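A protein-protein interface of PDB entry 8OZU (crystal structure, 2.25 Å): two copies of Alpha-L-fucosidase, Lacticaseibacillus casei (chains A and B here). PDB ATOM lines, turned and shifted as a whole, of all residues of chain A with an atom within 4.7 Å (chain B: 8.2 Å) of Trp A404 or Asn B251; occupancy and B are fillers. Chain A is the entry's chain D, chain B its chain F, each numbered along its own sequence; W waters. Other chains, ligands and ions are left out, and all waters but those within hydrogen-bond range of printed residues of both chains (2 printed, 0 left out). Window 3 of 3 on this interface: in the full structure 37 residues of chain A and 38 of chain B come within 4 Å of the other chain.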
ATOM      1  N   ILE A 262      11.035  10.297  -5.070  1.00  0.00           N
ATOM      2  CA  ILE A 262      10.133  10.492  -3.944  1.00  0.00           C
ATOM      3  C   ILE A 262       9.431   9.186  -3.576  1.00  0.00           C
ATOM      4  O   ILE A 262       9.410   8.832  -2.378  1.00  0.00           O
ATOM      5  CB  ILE A 262       9.124  11.618  -4.218  1.00  0.00           C
ATOM      6  CG1 ILE A 262       9.857  12.959  -4.277  1.00  0.00           C
ATOM      7  CG2 ILE A 262       8.037  11.609  -3.165  1.00  0.00           C
ATOM      8  CD1 ILE A 262       9.046  14.088  -4.909  1.00  0.00           C
ATOM      9  N   ARG A 300      11.860  19.553  -0.830  1.00  0.00           N
ATOM     10  CA  ARG A 300      10.508  20.026  -0.579  1.00  0.00           C
ATOM     11  C   ARG A 300       9.635  18.899  -0.022  1.00  0.00           C
ATOM     12  O   ARG A 300       8.889  19.143   0.925  1.00  0.00           O
ATOM     13  CB  ARG A 300       9.856  20.601  -1.835  1.00  0.00           C
ATOM     14  CG  ARG A 300      10.443  21.913  -2.282  1.00  0.00           C
ATOM     15  CD  ARG A 300       9.727  22.387  -3.530  1.00  0.00           C
ATOM     16  NE  ARG A 300      10.158  23.733  -3.878  1.00  0.00           N
ATOM     17  CZ  ARG A 300       9.722  24.855  -3.302  1.00  0.00           C
ATOM     18  NH1 ARG A 300       8.682  24.869  -2.470  1.00  0.00           N
ATOM     19  NH2 ARG A 300      10.292  25.987  -3.667  1.00  0.00           N
ATOM     20  N   TRP A 301       9.764  17.689  -0.597  1.00  0.00           N
ATOM     21  CA  TRP A 301       8.923  16.597  -0.139  1.00  0.00           C
ATOM     22  C   TRP A 301       9.294  16.217   1.307  1.00  0.00           C
ATOM     23  O   TRP A 301       8.402  16.069   2.147  1.00  0.00           O
ATOM     24  CB  TRP A 301       8.996  15.377  -1.061  1.00  0.00           C
ATOM     25  CG  TRP A 301       8.035  14.289  -0.684  1.00  0.00           C
ATOM     26  CD1 TRP A 301       6.720  14.211  -1.040  1.00  0.00           C
ATOM     27  CD2 TRP A 301       8.262  13.163   0.182  1.00  0.00           C
ATOM     28  NE1 TRP A 301       6.134  13.097  -0.501  1.00  0.00           N
ATOM     29  CE2 TRP A 301       7.051  12.445   0.269  1.00  0.00           C
ATOM     30  CE3 TRP A 301       9.378  12.663   0.854  1.00  0.00           C
ATOM     31  CZ2 TRP A 301       6.911  11.281   1.019  1.00  0.00           C
ATOM     32  CZ3 TRP A 301       9.245  11.515   1.601  1.00  0.00           C
ATOM     33  CH2 TRP A 301       8.027  10.832   1.682  1.00  0.00           C
ATOM     34  N   MET A 304       8.017  18.469   4.019  1.00  0.00           N
ATOM     35  CA  MET A 304       6.581  18.279   4.248  1.00  0.00           C
ATOM     36  C   MET A 304       6.351  16.971   5.023  1.00  0.00           C
ATOM     37  O   MET A 304       5.507  16.921   5.936  1.00  0.00           O
ATOM     38  CB  MET A 304       5.863  18.255   2.899  1.00  0.00           C
ATOM     39  CG  MET A 304       4.399  17.871   2.953  1.00  0.00           C
ATOM     40  SD  MET A 304       4.042  16.064   3.095  1.00  0.00           S
ATOM     41  CE  MET A 304       4.507  15.487   1.477  1.00  0.00           C
ATOM     42  N   ASP A 375       0.313  18.633   3.881  1.00  0.00           N
ATOM     43  CA  ASP A 375       0.828  19.715   3.043  1.00  0.00           C
ATOM     44  C   ASP A 375       0.044  21.018   3.234  1.00  0.00           C
ATOM     45  O   ASP A 375       0.594  22.099   3.064  1.00  0.00           O
ATOM     46  CB  ASP A 375       0.847  19.375   1.537  1.00  0.00           C
ATOM     47  CG  ASP A 375      -0.489  18.852   1.031  1.00  0.00           C
ATOM     48  OD1 ASP A 375      -0.766  17.653   1.267  1.00  0.00           O
ATOM     49  OD2 ASP A 375      -1.262  19.653   0.463  1.00  0.00           O
ATOM     50  N   TYR A 398      -4.889  17.199  -5.435  1.00  0.00           N
ATOM     51  CA  TYR A 398      -4.010  18.316  -5.157  1.00  0.00           C
ATOM     52  C   TYR A 398      -4.712  19.606  -5.560  1.00  0.00           C
ATOM     53  O   TYR A 398      -5.349  19.660  -6.617  1.00  0.00           O
ATOM     54  CB  TYR A 398      -2.728  18.173  -5.966  1.00  0.00           C
ATOM     55  CG  TYR A 398      -1.943  16.953  -5.596  1.00  0.00           C
ATOM     56  CD1 TYR A 398      -1.447  16.802  -4.314  1.00  0.00           C
ATOM     57  CD2 TYR A 398      -1.717  15.952  -6.521  1.00  0.00           C
ATOM     58  CE1 TYR A 398      -0.759  15.664  -3.941  1.00  0.00           C
ATOM     59  CE2 TYR A 398      -1.013  14.810  -6.181  1.00  0.00           C
ATOM     60  CZ  TYR A 398      -0.543  14.662  -4.883  1.00  0.00           C
ATOM     61  OH  TYR A 398       0.140  13.523  -4.509  1.00  0.00           O
ATOM     62  N   GLY A 401      -1.833  23.798  -9.073  1.00  0.00           N
ATOM     63  CA  GLY A 401      -0.549  24.421  -8.818  1.00  0.00           C
ATOM     64  C   GLY A 401       0.359  23.658  -7.869  1.00  0.00           C
ATOM     65  O   GLY A 401       1.462  24.104  -7.607  1.00  0.00           O
ATOM     66  N   SER A 402      -0.079  22.500  -7.379  1.00  0.00           N
ATOM     67  CA  SER A 402       0.809  21.670  -6.578  1.00  0.00           C
ATOM     68  C   SER A 402       0.631  20.186  -6.940  1.00  0.00           C
ATOM     69  O   SER A 402      -0.354  19.810  -7.586  1.00  0.00           O
ATOM     70  CB  SER A 402       0.580  21.971  -5.112  1.00  0.00           C
ATOM     71  OG  SER A 402      -0.618  21.340  -4.699  1.00  0.00           O
ATOM     72  N   ASP A 403       1.627  19.347  -6.581  1.00  0.00           N
ATOM     73  CA  ASP A 403       1.582  17.901  -6.789  1.00  0.00           C
ATOM     74  C   ASP A 403       2.722  17.244  -6.014  1.00  0.00           C
ATOM     75  O   ASP A 403       3.888  17.378  -6.393  1.00  0.00           O
ATOM     76  CB  ASP A 403       1.687  17.529  -8.264  1.00  0.00           C
ATOM     77  CG  ASP A 403       1.433  16.047  -8.576  1.00  0.00           C
ATOM     78  OD1 ASP A 403       1.776  15.145  -7.701  1.00  0.00           O
ATOM     79  OD2 ASP A 403       0.915  15.791  -9.721  1.00  0.00           O
ATOM     80  N   TRP A 404       2.396  16.588  -4.899  1.00  0.00           N
ATOM     81  CA  TRP A 404       3.400  16.103  -3.964  1.00  0.00           C
ATOM     82  C   TRP A 404       3.880  14.673  -4.258  1.00  0.00           C
ATOM     83  O   TRP A 404       4.743  14.187  -3.521  1.00  0.00           O
ATOM     84  CB  TRP A 404       2.833  16.190  -2.545  1.00  0.00           C
ATOM     85  CG  TRP A 404       2.660  17.612  -2.112  1.00  0.00           C
ATOM     86  CD1 TRP A 404       1.525  18.365  -2.239  1.00  0.00           C
ATOM     87  CD2 TRP A 404       3.657  18.458  -1.531  1.00  0.00           C
ATOM     88  NE1 TRP A 404       1.753  19.622  -1.782  1.00  0.00           N
ATOM     89  CE2 TRP A 404       3.044  19.709  -1.319  1.00  0.00           C
ATOM     90  CE3 TRP A 404       4.987  18.292  -1.155  1.00  0.00           C
ATOM     91  CZ2 TRP A 404       3.724  20.795  -0.745  1.00  0.00           C
ATOM     92  CZ3 TRP A 404       5.673  19.373  -0.606  1.00  0.00           C
ATOM     93  CH2 TRP A 404       5.039  20.601  -0.385  1.00  0.00           C
ATOM     94  N   VAL A 405       3.255  13.976  -5.247  1.00  0.00           N
ATOM     95  CA  VAL A 405       3.597  12.622  -5.626  1.00  0.00           C
ATOM     96  C   VAL A 405       3.176  11.586  -4.580  1.00  0.00           C
ATOM     97  O   VAL A 405       2.442  10.641  -4.915  1.00  0.00           O
ATOM     98  CB  VAL A 405       5.076  12.419  -6.008  1.00  0.00           C
ATOM     99  CG1 VAL A 405       5.302  11.013  -6.564  1.00  0.00           C
ATOM    100  CG2 VAL A 405       5.506  13.455  -7.037  1.00  0.00           C
ATOM    101  N   VAL A 406       3.702  11.663  -3.373  1.00  0.00           N
ATOM    102  CA  VAL A 406       3.191  10.863  -2.265  1.00  0.00           C
ATOM    103  C   VAL A 406       2.616  11.814  -1.238  1.00  0.00           C
ATOM    104  O   VAL A 406       3.354  12.622  -0.673  1.00  0.00           O
ATOM    105  CB  VAL A 406       4.293  10.016  -1.619  1.00  0.00           C
ATOM    106  CG1 VAL A 406       3.761   9.241  -0.416  1.00  0.00           C
ATOM    107  CG2 VAL A 406       4.916   9.091  -2.630  1.00  0.00           C
ATOM    108  N   MET B  28       2.831  34.067  -8.538  1.00  0.00           N
ATOM    109  CA  MET B  28       2.173  33.296  -7.503  1.00  0.00           C
ATOM    110  C   MET B  28       2.699  31.861  -7.451  1.00  0.00           C
ATOM    111  O   MET B  28       2.502  31.181  -6.435  1.00  0.00           O
ATOM    112  CB  MET B  28       0.676  33.237  -7.782  1.00  0.00           C
ATOM    113  CG  MET B  28       0.021  34.591  -7.930  1.00  0.00           C
ATOM    114  SD  MET B  28      -0.737  35.018  -6.361  1.00  0.00           S
ATOM    115  CE  MET B  28       0.699  35.601  -5.451  1.00  0.00           C
ATOM    116  N   ALA B  29       3.275  31.363  -8.569  1.00  0.00           N
ATOM    117  CA  ALA B  29       3.959  30.075  -8.598  1.00  0.00           C
ATOM    118  C   ALA B  29       3.016  28.922  -8.220  1.00  0.00           C
ATOM    119  O   ALA B  29       3.413  27.948  -7.566  1.00  0.00           O
ATOM    120  CB  ALA B  29       5.171  30.123  -7.694  1.00  0.00           C
ATOM    121  N   VAL B  30       1.765  29.025  -8.669  1.00  0.00           N
ATOM    122  CA  VAL B  30       0.813  27.938  -8.473  1.00  0.00           C
ATOM    123  C   VAL B  30       0.055  27.712  -9.792  1.00  0.00           C
ATOM    124  O   VAL B  30      -1.156  27.445  -9.790  1.00  0.00           O
ATOM    125  CB  VAL B  30      -0.124  28.199  -7.257  1.00  0.00           C
ATOM    126  CG1 VAL B  30       0.564  28.054  -5.896  1.00  0.00           C
ATOM    127  CG2 VAL B  30      -0.840  29.562  -7.345  1.00  0.00           C
ATOM    128  N   GLY B  31       0.771  27.815 -10.927  1.00  0.00           N
ATOM    129  CA  GLY B  31       0.201  27.502 -12.231  1.00  0.00           C
ATOM    130  C   GLY B  31      -0.421  28.702 -12.938  1.00  0.00           C
ATOM    131  O   GLY B  31      -0.883  29.658 -12.310  1.00  0.00           O
ATOM    132  N   ASN B 243       6.872  19.339 -15.567  1.00  0.00           N
ATOM    133  CA  ASN B 243       6.024  18.759 -14.518  1.00  0.00           C
ATOM    134  C   ASN B 243       4.573  18.767 -14.999  1.00  0.00           C
ATOM    135  O   ASN B 243       4.340  18.517 -16.187  1.00  0.00           O
ATOM    136  CB  ASN B 243       6.285  19.436 -13.180  1.00  0.00           C
ATOM    137  CG  ASN B 243       6.048  20.930 -13.185  1.00  0.00           C
ATOM    138  OD1 ASN B 243       5.470  21.503 -14.113  1.00  0.00           O
ATOM    139  ND2 ASN B 243       6.495  21.565 -12.111  1.00  0.00           N
ATOM    140  N   HIS B 245       2.421  21.445 -14.768  1.00  0.00           N
ATOM    141  CA  HIS B 245       1.892  22.766 -15.079  1.00  0.00           C
ATOM    142  C   HIS B 245       2.773  23.439 -16.120  1.00  0.00           C
ATOM    143  O   HIS B 245       3.885  23.027 -16.346  1.00  0.00           O
ATOM    144  CB  HIS B 245       1.768  23.591 -13.799  1.00  0.00           C
ATOM    145  CG  HIS B 245       0.891  22.970 -12.785  1.00  0.00           C
ATOM    146  ND1 HIS B 245       1.321  21.978 -11.923  1.00  0.00           N
ATOM    147  CD2 HIS B 245      -0.404  23.192 -12.508  1.00  0.00           C
ATOM    148  CE1 HIS B 245       0.301  21.602 -11.145  1.00  0.00           C
ATOM    149  NE2 HIS B 245      -0.774  22.260 -11.529  1.00  0.00           N
ATOM    150  N   ILE B 248       5.092  28.379 -13.880  1.00  0.00           N
ATOM    151  CA  ILE B 248       5.851  27.871 -12.765  1.00  0.00           C
ATOM    152  C   ILE B 248       4.910  27.467 -11.624  1.00  0.00           C
ATOM    153  O   ILE B 248       3.894  28.105 -11.347  1.00  0.00           O
ATOM    154  CB  ILE B 248       6.937  28.892 -12.364  1.00  0.00           C
ATOM    155  CG1 ILE B 248       7.924  28.290 -11.358  1.00  0.00           C
ATOM    156  CG2 ILE B 248       6.340  30.209 -11.874  1.00  0.00           C
ATOM    157  CD1 ILE B 248       9.145  29.156 -11.049  1.00  0.00           C
ATOM    158  N   ALA B 249       5.307  26.407 -10.929  1.00  0.00           N
ATOM    159  CA  ALA B 249       4.493  25.801  -9.890  1.00  0.00           C
ATOM    160  C   ALA B 249       5.402  25.167  -8.852  1.00  0.00           C
ATOM    161  O   ALA B 249       5.873  24.054  -9.024  1.00  0.00           O
ATOM    162  CB  ALA B 249       3.583  24.763 -10.490  1.00  0.00           C
ATOM    163  N   ALA B 250       5.660  25.908  -7.785  1.00  0.00           N
ATOM    164  CA  ALA B 250       6.775  25.596  -6.900  1.00  0.00           C
ATOM    165  C   ALA B 250       6.580  24.266  -6.183  1.00  0.00           C
ATOM    166  O   ALA B 250       7.570  23.600  -5.885  1.00  0.00           O
ATOM    167  CB  ALA B 250       6.937  26.708  -5.896  1.00  0.00           C
ATOM    168  N   ASN B 251       5.328  23.930  -5.815  1.00  0.00           N
ATOM    169  CA  ASN B 251       5.122  22.683  -5.080  1.00  0.00           C
ATOM    170  C   ASN B 251       4.558  21.589  -5.982  1.00  0.00           C
ATOM    171  O   ASN B 251       3.945  20.622  -5.512  1.00  0.00           O
ATOM    172  CB  ASN B 251       4.245  22.856  -3.849  1.00  0.00           C
ATOM    173  CG  ASN B 251       4.956  23.627  -2.771  1.00  0.00           C
ATOM    174  OD1 ASN B 251       6.142  23.417  -2.472  1.00  0.00           O
ATOM    175  ND2 ASN B 251       4.204  24.535  -2.182  1.00  0.00           N
ATOM    176  N   ASP B 252       4.807  21.713  -7.285  1.00  0.00           N
ATOM    177  CA  ASP B 252       4.617  20.604  -8.199  1.00  0.00           C
ATOM    178  C   ASP B 252       5.944  19.860  -8.328  1.00  0.00           C
ATOM    179  O   ASP B 252       6.807  20.295  -9.069  1.00  0.00           O
ATOM    180  CB  ASP B 252       4.127  21.125  -9.555  1.00  0.00           C
ATOM    181  CG  ASP B 252       3.951  20.053 -10.598  1.00  0.00           C
ATOM    182  OD1 ASP B 252       4.291  18.846 -10.299  1.00  0.00           O
ATOM    183  OD2 ASP B 252       3.457  20.430 -11.700  1.00  0.00           O
ATOM    184  N   LEU B 253       6.070  18.743  -7.632  1.00  0.00           N
ATOM    185  CA  LEU B 253       7.287  17.951  -7.608  1.00  0.00           C
ATOM    186  C   LEU B 253       7.201  16.829  -8.632  1.00  0.00           C
ATOM    187  O   LEU B 253       8.130  16.019  -8.725  1.00  0.00           O
ATOM    188  CB  LEU B 253       7.449  17.333  -6.212  1.00  0.00           C
ATOM    189  CG  LEU B 253       7.267  18.309  -5.052  1.00  0.00           C
ATOM    190  CD1 LEU B 253       7.581  17.676  -3.716  1.00  0.00           C
ATOM    191  CD2 LEU B 253       8.118  19.544  -5.267  1.00  0.00           C
ATOM    192  N   ASN B 254       6.091  16.773  -9.380  1.00  0.00           N
ATOM    193  CA  ASN B 254       5.821  15.618 -10.219  1.00  0.00           C
ATOM    194  C   ASN B 254       6.469  15.845 -11.586  1.00  0.00           C
ATOM    195  O   ASN B 254       5.810  16.005 -12.610  1.00  0.00           O
ATOM    196  CB  ASN B 254       4.326  15.382 -10.327  1.00  0.00           C
ATOM    197  CG  ASN B 254       3.979  14.120 -11.089  1.00  0.00           C
ATOM    198  OD1 ASN B 254       4.822  13.265 -11.356  1.00  0.00           O
ATOM    199  ND2 ASN B 254       2.711  13.942 -11.378  1.00  0.00           N
ATOM    200  N   TYR B 255       7.800  15.877 -11.573  1.00  0.00           N
ATOM    201  CA  TYR B 255       8.611  16.066 -12.761  1.00  0.00           C
ATOM    202  C   TYR B 255       8.786  14.719 -13.480  1.00  0.00           C
ATOM    203  O   TYR B 255       8.813  13.622 -12.903  1.00  0.00           O
ATOM    204  CB  TYR B 255       9.973  16.684 -12.410  1.00  0.00           C
ATOM    205  CG  TYR B 255      10.003  18.188 -12.239  1.00  0.00           C
ATOM    206  CD1 TYR B 255       9.516  18.798 -11.107  1.00  0.00           C
ATOM    207  CD2 TYR B 255      10.521  19.011 -13.219  1.00  0.00           C
ATOM    208  CE1 TYR B 255       9.580  20.170 -10.922  1.00  0.00           C
ATOM    209  CE2 TYR B 255      10.607  20.383 -13.070  1.00  0.00           C
ATOM    210  CZ  TYR B 255      10.115  20.971 -11.914  1.00  0.00           C
ATOM    211  OH  TYR B 255      10.125  22.323 -11.708  1.00  0.00           O
HETATM  212  O   HOH W   1       2.994  25.244  -6.109  1.00  0.00           O
HETATM  213  O   HOH W   2       1.338  12.942  -8.556  1.00  0.00           O
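NE of Arg A300 lies within hydrogen-bond range of O of Ala B250, at 3.3 Å.
The guanidinium group (NH1) of Arg A300 sits at hydrogen-bond distance from the side-chain amide oxygen (OD1) of Asn B251 (2.9 Å).
The backbone NH (N) of Gly A401 lies within hydrogen-bond range of a ring nitrogen (NE2) of His B245 (3.1 Å).
The backbone NH (N) of Asp A403 is in hydrogen-bond range of the backbone carbonyl oxygen (O) of Asn B251.
The backbone carbonyl oxygen of Asp A403 is in hydrogen-bond range of the backbone NH of Leu B253, at 2.9 Å.
The side-chain amide nitrogen (ND2) of Asn B254 lies within hydrogen-bond range of the side-chain carboxylate (OD2) of Asp A403, at 3.1 Å.
NE1 of Trp A301 sits close to O of Trp A404 (3.5 Å).
The indole nitrogen (NE1) of Trp A301 lies within hydrogen-bond range of the backbone carbonyl oxygen (O) of Val A406, at 2.8 Å.
The side-chain hydroxyl (OH) of Tyr A398 is in hydrogen-bond range of the backbone NH (N) of Val A405, 3.2 Å away.
The side-chain amide oxygen (OD1) of Asn B243 sits at hydrogen-bond distance from the backbone NH (N) of His B245 (3.1 Å).
ND1 of His B245 is in hydrogen-bond range of OD2 of Asp B252 (2.6 Å).
The backbone NH (N) of Asn B254 lies within hydrogen-bond range of the side-chain carboxylate (OD1) of Asp B252 (2.9 Å).
Leu B253 touches Ile A262 (CB to CD1, 3.8 Å).
Arg A300 touches Leu B253.
CD1 of Leu B253 touches CB of Trp A301 (3.8 Å).
CA of Gly A401 touches O of Val B30 (3.2 Å).
O of Gly A401 touches CB of Ala B249, 3.6 Å away.
Ser A402 touches His B245 (N to CE1, 3.9 Å).
Ser A402 touches Asn B251 (CA to O, 3.5 Å).
Asp A403 touches Asp B252.
CH2 of Trp A404 touches OD1 of Asn B251, 3.7 Å away.
Asn B254 touches Val A405.
No position is printed for both chains.
Of the 17 pairs that touch across the chains among the printed residues, none has its exchanged pair printed and touching as well.
Of the 14 printed residues of chain B, 8 touch a printed residue of chain A.
Printed residues of chain B that touch a printed residue of chain A: Val B30, His B245, Ala B249, Ala B250, Asn B251, Asp B252, Leu B253 and Asn B254.
Hydrophobic or aromatic side chains of chain B that line the printed part of chain A: His B245, Ala B249 and Leu B253.
Of the 12 printed residues of chain A, 8 touch a printed residue of chain B.
Hydrophobic or aromatic side chains of chain A that line the printed part of chain B: Ile A262, Trp A301, Trp A404 and Val A405.
Among the printed residues, 17 pairs touch across the chains.
Among the printed residues, no Asp or Glu carboxylate lies within 4 Å of a Lys or Arg side-chain nitrogen of the other chain.
Of chain B, only Asn B251 (3.7 Å) and Leu B253 (3.7 Å) come within 4 Å of Trp A404.
Of chain A, only Arg A300 (2.9 Å), Ser A402 (3.5 Å), Asp A403 (2.9 Å) and Trp A404 (3.7 Å) come within 4 Å of Asn B251.
Printed residues of chain B within 4 Å of Trp A301: Leu B253 (3.8 Å).
Of the printed residues of chain B, Val A405 touches Asn B254 (3.9 Å).
Of the printed residues of chain A, His B245 touches Gly A401 and Ser A402.
Of the printed residues of chain A, Ala B250 touches Arg A300 (3.3 Å).
Asn B243 touches none of the printed residues of chain A.
Gly B31 touches none of the printed residues of chain A.
The nearest residue of chain B that does not touch Trp A404 is Asp B252 (5.7 Å).
Water W2 bridges the side-chain carboxylate (OD1) of Asp A403 (2.4 Å) and the side-chain amide nitrogen (ND2) of Asn B254 (3.3 Å).
Water W1 lies within hydrogen-bond range of O of Gly A401 (2.4 Å), N of Asn B251 (2.7 Å), O of Ala B29 (3.1 Å) and N of Ala B250 (3.2 Å).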
